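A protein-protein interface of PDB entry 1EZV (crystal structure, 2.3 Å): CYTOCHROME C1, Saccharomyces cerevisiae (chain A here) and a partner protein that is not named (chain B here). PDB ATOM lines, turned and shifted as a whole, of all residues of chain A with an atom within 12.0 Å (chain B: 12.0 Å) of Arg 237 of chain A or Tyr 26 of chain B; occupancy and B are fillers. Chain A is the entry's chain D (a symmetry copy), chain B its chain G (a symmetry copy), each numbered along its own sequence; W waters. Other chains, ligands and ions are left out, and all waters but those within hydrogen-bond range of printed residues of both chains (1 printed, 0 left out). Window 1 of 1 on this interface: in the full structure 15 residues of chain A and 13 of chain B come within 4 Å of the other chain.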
ATOM      1  N   LYS A 228      -9.209 -23.791  17.924  1.00  0.00           N
ATOM      2  CA  LYS A 228     -10.019 -22.925  17.074  1.00  0.00           C
ATOM      3  C   LYS A 228     -11.500 -23.031  17.425  1.00  0.00           C
ATOM      4  O   LYS A 228     -12.179 -22.014  17.570  1.00  0.00           O
ATOM      5  CB  LYS A 228      -9.807 -23.275  15.600  1.00  0.00           C
ATOM      6  CG  LYS A 228      -8.469 -22.816  15.034  1.00  0.00           C
ATOM      7  CD  LYS A 228      -8.305 -23.256  13.579  1.00  0.00           C
ATOM      8  CE  LYS A 228      -7.027 -22.693  12.959  1.00  0.00           C
ATOM      9  NZ  LYS A 228      -7.000 -21.194  12.940  1.00  0.00           N
ATOM     10  N   PHE A 229     -11.966 -24.255  17.675  1.00  0.00           N
ATOM     11  CA  PHE A 229     -13.350 -24.480  18.061  1.00  0.00           C
ATOM     12  C   PHE A 229     -13.654 -23.782  19.377  1.00  0.00           C
ATOM     13  O   PHE A 229     -14.628 -23.035  19.474  1.00  0.00           O
ATOM     14  CB  PHE A 229     -13.650 -25.984  18.186  1.00  0.00           C
ATOM     15  CG  PHE A 229     -15.042 -26.292  18.705  1.00  0.00           C
ATOM     16  CD1 PHE A 229     -15.252 -26.563  20.053  1.00  0.00           C
ATOM     17  CD2 PHE A 229     -16.136 -26.303  17.844  1.00  0.00           C
ATOM     18  CE1 PHE A 229     -16.529 -26.838  20.541  1.00  0.00           C
ATOM     19  CE2 PHE A 229     -17.426 -26.578  18.323  1.00  0.00           C
ATOM     20  CZ  PHE A 229     -17.619 -26.844  19.675  1.00  0.00           C
ATOM     21  N   LYS A 230     -12.797 -23.992  20.374  1.00  0.00           N
ATOM     22  CA  LYS A 230     -13.011 -23.403  21.691  1.00  0.00           C
ATOM     23  C   LYS A 230     -12.892 -21.881  21.710  1.00  0.00           C
ATOM     24  O   LYS A 230     -13.472 -21.228  22.578  1.00  0.00           O
ATOM     25  CB  LYS A 230     -12.059 -24.032  22.713  1.00  0.00           C
ATOM     26  CG  LYS A 230     -12.483 -25.433  23.114  1.00  0.00           C
ATOM     27  CD  LYS A 230     -11.636 -26.001  24.233  1.00  0.00           C
ATOM     28  CE  LYS A 230     -12.085 -27.420  24.602  1.00  0.00           C
ATOM     29  NZ  LYS A 230     -13.575 -27.546  24.739  1.00  0.00           N
ATOM     30  N   TRP A 231     -12.258 -21.320  20.682  1.00  0.00           N
ATOM     31  CA  TRP A 231     -12.095 -19.874  20.574  1.00  0.00           C
ATOM     32  C   TRP A 231     -13.092 -19.168  19.626  1.00  0.00           C
ATOM     33  O   TRP A 231     -13.136 -17.929  19.593  1.00  0.00           O
ATOM     34  CB  TRP A 231     -10.657 -19.537  20.143  1.00  0.00           C
ATOM     35  CG  TRP A 231      -9.683 -19.461  21.277  1.00  0.00           C
ATOM     36  CD1 TRP A 231      -9.145 -20.509  21.966  1.00  0.00           C
ATOM     37  CD2 TRP A 231      -9.145 -18.272  21.872  1.00  0.00           C
ATOM     38  NE1 TRP A 231      -8.308 -20.048  22.954  1.00  0.00           N
ATOM     39  CE2 TRP A 231      -8.295 -18.678  22.923  1.00  0.00           C
ATOM     40  CE3 TRP A 231      -9.316 -16.901  21.631  1.00  0.00           C
ATOM     41  CZ2 TRP A 231      -7.621 -17.762  23.744  1.00  0.00           C
ATOM     42  CZ3 TRP A 231      -8.646 -15.989  22.450  1.00  0.00           C
ATOM     43  CH2 TRP A 231      -7.813 -16.427  23.495  1.00  0.00           C
ATOM     44  N   ALA A 232     -13.915 -19.937  18.906  1.00  0.00           N
ATOM     45  CA  ALA A 232     -14.750 -19.374  17.832  1.00  0.00           C
ATOM     46  C   ALA A 232     -15.738 -18.310  18.311  1.00  0.00           C
ATOM     47  O   ALA A 232     -15.946 -17.304  17.636  1.00  0.00           O
ATOM     48  CB  ALA A 232     -15.495 -20.486  17.078  1.00  0.00           C
ATOM     49  N   GLY A 233     -16.289 -18.492  19.503  1.00  0.00           N
ATOM     50  CA  GLY A 233     -17.148 -17.469  20.069  1.00  0.00           C
ATOM     51  C   GLY A 233     -16.442 -16.145  20.298  1.00  0.00           C
ATOM     52  O   GLY A 233     -17.029 -15.080  20.085  1.00  0.00           O
ATOM     53  N   ILE A 234     -15.180 -16.208  20.723  1.00  0.00           N
ATOM     54  CA  ILE A 234     -14.413 -15.008  21.075  1.00  0.00           C
ATOM     55  C   ILE A 234     -13.871 -14.311  19.823  1.00  0.00           C
ATOM     56  O   ILE A 234     -13.981 -13.092  19.683  1.00  0.00           O
ATOM     57  CB  ILE A 234     -13.239 -15.365  22.053  1.00  0.00           C
ATOM     58  CG1 ILE A 234     -13.806 -15.745  23.424  1.00  0.00           C
ATOM     59  CG2 ILE A 234     -12.259 -14.198  22.192  1.00  0.00           C
ATOM     60  CD1 ILE A 234     -14.591 -14.638  24.111  1.00  0.00           C
ATOM     61  N   LYS A 235     -13.436 -15.105  18.852  1.00  0.00           N
ATOM     62  CA  LYS A 235     -12.839 -14.565  17.643  1.00  0.00           C
ATOM     63  C   LYS A 235     -13.840 -13.829  16.759  1.00  0.00           C
ATOM     64  O   LYS A 235     -13.488 -12.840  16.113  1.00  0.00           O
ATOM     65  CB  LYS A 235     -12.165 -15.679  16.847  1.00  0.00           C
ATOM     66  CG  LYS A 235     -10.902 -16.208  17.493  1.00  0.00           C
ATOM     67  CD  LYS A 235      -9.662 -15.556  16.907  1.00  0.00           C
ATOM     68  CE  LYS A 235      -8.413 -15.980  17.664  1.00  0.00           C
ATOM     69  NZ  LYS A 235      -7.163 -15.607  16.952  1.00  0.00           N
ATOM     70  N   THR A 236     -15.082 -14.302  16.728  1.00  0.00           N
ATOM     71  CA  THR A 236     -16.094 -13.685  15.876  1.00  0.00           C
ATOM     72  C   THR A 236     -17.032 -12.760  16.648  1.00  0.00           C
ATOM     73  O   THR A 236     -17.962 -12.201  16.089  1.00  0.00           O
ATOM     74  CB  THR A 236     -16.911 -14.754  15.120  1.00  0.00           C
ATOM     75  OG1 THR A 236     -17.491 -15.668  16.058  1.00  0.00           O
ATOM     76  CG2 THR A 236     -16.003 -15.521  14.151  1.00  0.00           C
ATOM     77  N   ARG A 237     -16.715 -12.541  17.917  1.00  0.00           N
ATOM     78  CA  ARG A 237     -17.420 -11.599  18.782  1.00  0.00           C
ATOM     79  C   ARG A 237     -17.463 -10.209  18.131  1.00  0.00           C
ATOM     80  O   ARG A 237     -16.510  -9.812  17.459  1.00  0.00           O
ATOM     81  CB  ARG A 237     -16.678 -11.542  20.122  1.00  0.00           C
ATOM     82  CG  ARG A 237     -17.349 -10.777  21.233  1.00  0.00           C
ATOM     83  CD  ARG A 237     -16.641 -11.063  22.560  1.00  0.00           C
ATOM     84  NE  ARG A 237     -15.187 -10.902  22.472  1.00  0.00           N
ATOM     85  CZ  ARG A 237     -14.414 -10.473  23.470  1.00  0.00           C
ATOM     86  NH1 ARG A 237     -13.126 -10.235  23.256  1.00  0.00           N
ATOM     87  NH2 ARG A 237     -14.908 -10.332  24.694  1.00  0.00           N
ATOM     88  N   LYS A 238     -18.590  -9.509  18.279  1.00  0.00           N
ATOM     89  CA  LYS A 238     -18.756  -8.168  17.709  1.00  0.00           C
ATOM     90  C   LYS A 238     -19.234  -7.162  18.744  1.00  0.00           C
ATOM     91  O   LYS A 238     -20.131  -7.454  19.533  1.00  0.00           O
ATOM     92  CB  LYS A 238     -19.753  -8.192  16.549  1.00  0.00           C
ATOM     93  CG  LYS A 238     -19.563  -9.352  15.596  1.00  0.00           C
ATOM     94  CD  LYS A 238     -19.547  -8.904  14.151  1.00  0.00           C
ATOM     95  CE  LYS A 238     -19.251 -10.080  13.228  1.00  0.00           C
ATOM     96  NZ  LYS A 238     -19.590  -9.782  11.801  1.00  0.00           N
ATOM     97  N   PHE A 239     -18.677  -5.956  18.689  1.00  0.00           N
ATOM     98  CA  PHE A 239     -19.060  -4.879  19.601  1.00  0.00           C
ATOM     99  C   PHE A 239     -19.795  -3.733  18.870  1.00  0.00           C
ATOM    100  O   PHE A 239     -19.598  -3.519  17.666  1.00  0.00           O
ATOM    101  CB  PHE A 239     -17.816  -4.327  20.312  1.00  0.00           C
ATOM    102  CG  PHE A 239     -17.191  -5.285  21.291  1.00  0.00           C
ATOM    103  CD1 PHE A 239     -16.302  -6.271  20.857  1.00  0.00           C
ATOM    104  CD2 PHE A 239     -17.501  -5.218  22.646  1.00  0.00           C
ATOM    105  CE1 PHE A 239     -15.734  -7.181  21.758  1.00  0.00           C
ATOM    106  CE2 PHE A 239     -16.944  -6.123  23.557  1.00  0.00           C
ATOM    107  CZ  PHE A 239     -16.059  -7.108  23.106  1.00  0.00           C
ATOM    108  N   VAL A 240     -20.717  -3.074  19.575  1.00  0.00           N
ATOM    109  CA  VAL A 240     -21.283  -1.804  19.123  1.00  0.00           C
ATOM    110  C   VAL A 240     -21.276  -0.761  20.240  1.00  0.00           C
ATOM    111  O   VAL A 240     -21.574  -1.062  21.391  1.00  0.00           O
ATOM    112  CB  VAL A 240     -22.741  -1.956  18.615  1.00  0.00           C
ATOM    113  CG1 VAL A 240     -22.780  -2.810  17.374  1.00  0.00           C
ATOM    114  CG2 VAL A 240     -23.620  -2.546  19.702  1.00  0.00           C
ATOM    115  N   PHE A 241     -20.959   0.477  19.885  1.00  0.00           N
ATOM    116  CA  PHE A 241     -20.961   1.571  20.847  1.00  0.00           C
ATOM    117  C   PHE A 241     -22.099   2.554  20.535  1.00  0.00           C
ATOM    118  O   PHE A 241     -22.283   2.965  19.389  1.00  0.00           O
ATOM    119  CB  PHE A 241     -19.611   2.285  20.805  1.00  0.00           C
ATOM    120  CG  PHE A 241     -19.461   3.385  21.820  1.00  0.00           C
ATOM    121  CD1 PHE A 241     -19.796   3.175  23.158  1.00  0.00           C
ATOM    122  CD2 PHE A 241     -18.907   4.608  21.454  1.00  0.00           C
ATOM    123  CE1 PHE A 241     -19.579   4.161  24.120  1.00  0.00           C
ATOM    124  CE2 PHE A 241     -18.685   5.607  22.410  1.00  0.00           C
ATOM    125  CZ  PHE A 241     -19.021   5.380  23.748  1.00  0.00           C
ATOM    126  N   ASN A 242     -22.934   2.809  21.539  1.00  0.00           N
ATOM    127  CA  ASN A 242     -23.940   3.860  21.467  1.00  0.00           C
ATOM    128  C   ASN A 242     -23.679   4.840  22.604  1.00  0.00           C
ATOM    129  O   ASN A 242     -23.967   4.546  23.762  1.00  0.00           O
ATOM    130  CB  ASN A 242     -25.350   3.269  21.596  1.00  0.00           C
ATOM    131  CG  ASN A 242     -25.751   2.453  20.385  1.00  0.00           C
ATOM    132  OD1 ASN A 242     -25.601   2.896  19.251  1.00  0.00           O
ATOM    133  ND2 ASN A 242     -26.249   1.249  20.618  1.00  0.00           N
ATOM    134  N   TRP B  12     -12.928 -10.775  38.936  1.00  0.00           N
ATOM    135  CA  TRP B  12     -14.263 -10.729  38.341  1.00  0.00           C
ATOM    136  C   TRP B  12     -15.277  -9.958  39.187  1.00  0.00           C
ATOM    137  O   TRP B  12     -15.488 -10.273  40.367  1.00  0.00           O
ATOM    138  CB  TRP B  12     -14.768 -12.150  38.105  1.00  0.00           C
ATOM    139  CG  TRP B  12     -13.857 -12.948  37.240  1.00  0.00           C
ATOM    140  CD1 TRP B  12     -13.074 -13.989  37.625  1.00  0.00           C
ATOM    141  CD2 TRP B  12     -13.641 -12.776  35.835  1.00  0.00           C
ATOM    142  NE1 TRP B  12     -12.383 -14.485  36.546  1.00  0.00           N
ATOM    143  CE2 TRP B  12     -12.718 -13.765  35.434  1.00  0.00           C
ATOM    144  CE3 TRP B  12     -14.149 -11.891  34.873  1.00  0.00           C
ATOM    145  CZ2 TRP B  12     -12.293 -13.902  34.098  1.00  0.00           C
ATOM    146  CZ3 TRP B  12     -13.730 -12.029  33.543  1.00  0.00           C
ATOM    147  CH2 TRP B  12     -12.815 -13.032  33.172  1.00  0.00           C
ATOM    148  N   MET B  15     -12.578  -5.602  38.475  1.00  0.00           N
ATOM    149  CA  MET B  15     -11.309  -5.768  37.777  1.00  0.00           C
ATOM    150  C   MET B  15     -10.412  -4.551  37.917  1.00  0.00           C
ATOM    151  O   MET B  15      -9.188  -4.664  37.807  1.00  0.00           O
ATOM    152  CB  MET B  15     -11.544  -6.059  36.296  1.00  0.00           C
ATOM    153  CG  MET B  15     -10.422  -6.865  35.658  1.00  0.00           C
ATOM    154  SD  MET B  15     -10.298  -8.525  36.359  1.00  0.00           S
ATOM    155  CE  MET B  15     -11.666  -9.331  35.528  1.00  0.00           C
ATOM    156  N   GLN B  20     -18.011   1.018  32.601  1.00  0.00           N
ATOM    157  CA  GLN B  20     -18.365   0.832  31.198  1.00  0.00           C
ATOM    158  C   GLN B  20     -19.854   1.051  31.007  1.00  0.00           C
ATOM    159  O   GLN B  20     -20.665   0.523  31.763  1.00  0.00           O
ATOM    160  CB  GLN B  20     -17.990  -0.581  30.722  1.00  0.00           C
ATOM    161  CG  GLN B  20     -16.491  -0.842  30.608  1.00  0.00           C
ATOM    162  CD  GLN B  20     -16.179  -2.236  30.088  1.00  0.00           C
ATOM    163  OE1 GLN B  20     -16.942  -2.801  29.306  1.00  0.00           O
ATOM    164  NE2 GLN B  20     -15.059  -2.801  30.528  1.00  0.00           N
ATOM    165  N   GLY B  22     -22.719   1.879  27.537  1.00  0.00           N
ATOM    166  CA  GLY B  22     -22.937   2.159  26.131  1.00  0.00           C
ATOM    167  C   GLY B  22     -22.405   1.113  25.173  1.00  0.00           C
ATOM    168  O   GLY B  22     -22.772   1.107  23.993  1.00  0.00           O
ATOM    169  N   ILE B  23     -21.481   0.279  25.645  1.00  0.00           N
ATOM    170  CA  ILE B  23     -20.921  -0.791  24.816  1.00  0.00           C
ATOM    171  C   ILE B  23     -21.784  -2.047  24.942  1.00  0.00           C
ATOM    172  O   ILE B  23     -22.084  -2.492  26.048  1.00  0.00           O
ATOM    173  CB  ILE B  23     -19.473  -1.127  25.245  1.00  0.00           C
ATOM    174  CG1 ILE B  23     -18.610   0.137  25.201  1.00  0.00           C
ATOM    175  CG2 ILE B  23     -18.892  -2.217  24.345  1.00  0.00           C
ATOM    176  CD1 ILE B  23     -17.402   0.104  26.119  1.00  0.00           C
ATOM    177  N   THR B  24     -22.185  -2.599  23.805  1.00  0.00           N
ATOM    178  CA  THR B  24     -22.999  -3.806  23.763  1.00  0.00           C
ATOM    179  C   THR B  24     -22.269  -4.842  22.913  1.00  0.00           C
ATOM    180  O   THR B  24     -21.864  -4.544  21.789  1.00  0.00           O
ATOM    181  CB  THR B  24     -24.385  -3.504  23.126  1.00  0.00           C
ATOM    182  OG1 THR B  24     -25.087  -2.573  23.954  1.00  0.00           O
ATOM    183  CG2 THR B  24     -25.219  -4.768  22.974  1.00  0.00           C
ATOM    184  N   SER B  25     -22.095  -6.053  23.441  1.00  0.00           N
ATOM    185  CA  SER B  25     -21.384  -7.081  22.690  1.00  0.00           C
ATOM    186  C   SER B  25     -22.294  -8.223  22.288  1.00  0.00           C
ATOM    187  O   SER B  25     -23.307  -8.477  22.932  1.00  0.00           O
ATOM    188  CB  SER B  25     -20.194  -7.616  23.492  1.00  0.00           C
ATOM    189  OG  SER B  25     -20.625  -8.360  24.616  1.00  0.00           O
ATOM    190  N   TYR B  26     -21.933  -8.896  21.205  1.00  0.00           N
ATOM    191  CA  TYR B  26     -22.728 -10.002  20.688  1.00  0.00           C
ATOM    192  C   TYR B  26     -21.791 -11.150  20.356  1.00  0.00           C
ATOM    193  O   TYR B  26     -20.682 -10.918  19.873  1.00  0.00           O
ATOM    194  CB  TYR B  26     -23.473  -9.587  19.412  1.00  0.00           C
ATOM    195  CG  TYR B  26     -24.398  -8.399  19.571  1.00  0.00           C
ATOM    196  CD1 TYR B  26     -23.911  -7.095  19.481  1.00  0.00           C
ATOM    197  CD2 TYR B  26     -25.775  -8.577  19.721  1.00  0.00           C
ATOM    198  CE1 TYR B  26     -24.766  -6.004  19.534  1.00  0.00           C
ATOM    199  CE2 TYR B  26     -26.644  -7.488  19.758  1.00  0.00           C
ATOM    200  CZ  TYR B  26     -26.133  -6.207  19.666  1.00  0.00           C
ATOM    201  OH  TYR B  26     -26.982  -5.121  19.692  1.00  0.00           O
ATOM    202  N   ALA B  27     -22.264 -12.379  20.534  1.00  0.00           N
ATOM    203  CA  ALA B  27     -21.498 -13.542  20.115  1.00  0.00           C
ATOM    204  C   ALA B  27     -22.422 -14.715  19.800  1.00  0.00           C
ATOM    205  O   ALA B  27     -23.585 -14.722  20.194  1.00  0.00           O
ATOM    206  CB  ALA B  27     -20.484 -13.934  21.209  1.00  0.00           C
ATOM    207  N   VAL B  28     -21.856 -15.751  19.189  1.00  0.00           N
ATOM    208  CA  VAL B  28     -22.625 -16.898  18.737  1.00  0.00           C
ATOM    209  C   VAL B  28     -21.874 -18.179  19.095  1.00  0.00           C
ATOM    210  O   VAL B  28     -20.662 -18.273  18.883  1.00  0.00           O
ATOM    211  CB  VAL B  28     -22.851 -16.841  17.196  1.00  0.00           C
ATOM    212  CG1 VAL B  28     -23.353 -18.182  16.680  1.00  0.00           C
ATOM    213  CG2 VAL B  28     -23.860 -15.747  16.857  1.00  0.00           C
ATOM    214  N   SER B  29     -22.606 -19.172  19.591  1.00  0.00           N
ATOM    215  CA  SER B  29     -22.016 -20.435  20.012  1.00  0.00           C
ATOM    216  C   SER B  29     -21.109 -21.020  18.933  1.00  0.00           C
ATOM    217  O   SER B  29     -21.452 -21.010  17.745  1.00  0.00           O
ATOM    218  CB  SER B  29     -23.108 -21.448  20.364  1.00  0.00           C
ATOM    219  OG  SER B  29     -22.555 -22.728  20.636  1.00  0.00           O
ATOM    220  N   PRO B  30     -19.906 -21.473  19.331  1.00  0.00           N
ATOM    221  CA  PRO B  30     -19.032 -22.283  18.478  1.00  0.00           C
ATOM    222  C   PRO B  30     -19.766 -23.467  17.874  1.00  0.00           C
ATOM    223  O   PRO B  30     -19.455 -23.891  16.766  1.00  0.00           O
ATOM    224  CB  PRO B  30     -17.928 -22.732  19.433  1.00  0.00           C
ATOM    225  CG  PRO B  30     -17.836 -21.604  20.406  1.00  0.00           C
ATOM    226  CD  PRO B  30     -19.263 -21.157  20.621  1.00  0.00           C
ATOM    227  N   ALA B  32     -22.809 -23.563  16.834  1.00  0.00           N
ATOM    228  CA  ALA B  32     -23.665 -23.096  15.748  1.00  0.00           C
ATOM    229  C   ALA B  32     -22.866 -22.596  14.548  1.00  0.00           C
ATOM    230  O   ALA B  32     -23.444 -22.177  13.544  1.00  0.00           O
ATOM    231  CB  ALA B  32     -24.584 -21.989  16.254  1.00  0.00           C
ATOM    232  N   GLN B  33     -21.542 -22.598  14.667  1.00  0.00           N
ATOM    233  CA  GLN B  33     -20.688 -22.021  13.638  1.00  0.00           C
ATOM    234  C   GLN B  33     -20.153 -23.081  12.698  1.00  0.00           C
ATOM    235  O   GLN B  33     -20.105 -24.265  13.034  1.00  0.00           O
ATOM    236  CB  GLN B  33     -19.521 -21.256  14.266  1.00  0.00           C
ATOM    237  CG  GLN B  33     -19.940 -20.046  15.080  1.00  0.00           C
ATOM    238  CD  GLN B  33     -18.759 -19.229  15.568  1.00  0.00           C
ATOM    239  OE1 GLN B  33     -17.731 -19.140  14.896  1.00  0.00           O
ATOM    240  NE2 GLN B  33     -18.906 -18.615  16.738  1.00  0.00           N
HETATM  241  O   HOH W   1     -19.293 -14.941  18.313  1.00  0.00           O
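The side-chain amide nitrogen (NE2) of Gln 33 of chain B sits at hydrogen-bond distance from the backbone carbonyl oxygen (O) of Ala 232 of chain A, at 3.4 Å.
The side-chain amide nitrogen (NE2) of Gln 33 of chain B lies within hydrogen-bond range of the side-chain hydroxyl (OG1) of Thr 236 of chain A, 3.3 Å away.
The backbone NH (N) of Tyr 26 of chain B is in hydrogen-bond range of the backbone carbonyl oxygen (O) of Lys 238 of chain A (2.8 Å).
The backbone carbonyl oxygen (O) of Thr 24 of chain B lies within hydrogen-bond range of the backbone NH (N) of Val 240 of chain A, 2.9 Å away.
The backbone NH (N) of Asn 242 of chain A lies within hydrogen-bond range of the backbone carbonyl oxygen (O) of Gly 22 of chain B (3.0 Å).
The backbone carbonyl oxygen (O) of Ala 232 of chain A is in hydrogen-bond range of the side-chain hydroxyl (OG1) of Thr 236 of chain A (2.7 Å).
O of Val 28 of chain B is in hydrogen-bond range of NE2 of Gln 33 of chain B, at 2.8 Å.
Among the printed residues, merely in contact across the chains: Phe 229 of chain A with Pro 30 of chain B (3.3 Å), Gly 233 of chain A with Ala 27 of chain B (3.8 Å), Gly 233 of chain A with Val 28 of chain B (3.8 Å), Gly 233 of chain A with Pro 30 of chain B (3.6 Å), Gly 233 of chain A with Gln 33 of chain B (3.8 Å), Arg 237 of chain A with Tyr 26 of chain B (3.5 Å), Lys 238 of chain A with Ser 25 of chain B (3.4 Å), Phe 239 of chain A with Ile 23 of chain B (3.7 Å), Phe 239 of chain A with Thr 24 of chain B (3.6 Å), Phe 239 of chain A with Ser 25 of chain B (3.6 Å), Val 240 of chain A with Gly 22 of chain B (3.6 Å), Val 240 of chain A with Ile 23 of chain B (3.5 Å), Val 240 of chain A with Tyr 26 of chain B (3.6 Å), Phe 241 of chain A with Gly 22 of chain B (3.7 Å) and Phe 241 of chain A with Ile 23 of chain B (3.8 Å).
Of chain B, only Tyr 26 (3.5 Å) comes within 4 Å of Arg 237 of chain A.
Of chain A, only Arg 237 (3.5 Å), Lys 238 (2.8 Å) and Val 240 (3.6 Å) come within 4 Å of Tyr 26 of chain B.
Of the printed residues of chain B, Gly 233 of chain A touches Ala 27 (3.8 Å), Val 28 (3.8 Å), Pro 30 (3.6 Å) and Gln 33 (3.8 Å).
No residue of chain B comes within 4 Å of Ile 234 of chain A.
Of chain B, only Ile 23 (3.7 Å), Thr 24 (3.6 Å) and Ser 25 (3.6 Å) come within 4 Å of Phe 239 of chain A.
Of chain A, only Phe 239 (3.6 Å) and Val 240 (2.9 Å) come within 4 Å of Thr 24 of chain B.
Ser 25 of chain B touches two residues of chain A.
Of the printed residues of chain A, Ala 27 of chain B touches Gly 233.
Of the printed residues of chain B, Asn 242 of chain A touches Gly 22 (3.0 Å).
Printed residues of chain A within 4 Å of Gln 33 of chain B: Ala 232 (3.4 Å), Gly 233 (3.8 Å) and Thr 236 (3.3 Å).
Of the printed residues of chain A, Pro 30 of chain B touches Phe 229 (3.3 Å) and Gly 233 (3.6 Å).
Printed residues of chain A within 4 Å of Ile 23 of chain B: Phe 239, Val 240 and Phe 241.
Of the printed residues of chain B, Phe 241 of chain A touches Gly 22 and Ile 23.
The nearest residue of chain B that does not touch Arg 237 of chain A is Ala 27 of chain B (4.4 Å).
The nearest residue of chain A that does not touch Tyr 26 of chain B is Thr 236 of chain A (4.8 Å).
The nearest printed residue of chain A that does not touch Val 28 of chain B is Ala 232 of chain A (5.0 Å).
Of the 15 printed residues of chain A, 10 touch a printed residue of chain B.
Printed residues of chain A that touch a printed residue of chain B: Phe 229, Ala 232, Gly 233, Thr 236, Arg 237, Lys 238, Phe 239, Val 240, Phe 241 and Asn 242.
Hydrophobic or aromatic side chains of chain A that line the printed part of chain B: Phe 229, Ala 232, Phe 239, Val 240 and Phe 241.
Among the printed residues, 20 pairs touch across the chains.
Among the printed residues, no Asp or Glu carboxylate lies within 4 Å of a Lys or Arg side-chain nitrogen of the other chain.
Water W1 lies within hydrogen-bond range of the backbone NH (N) of Val 28 of chain B, the backbone carbonyl oxygen (O) of Gly 233 of chain A and the side-chain hydroxyl (OG1) of Thr 236 of chain A.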
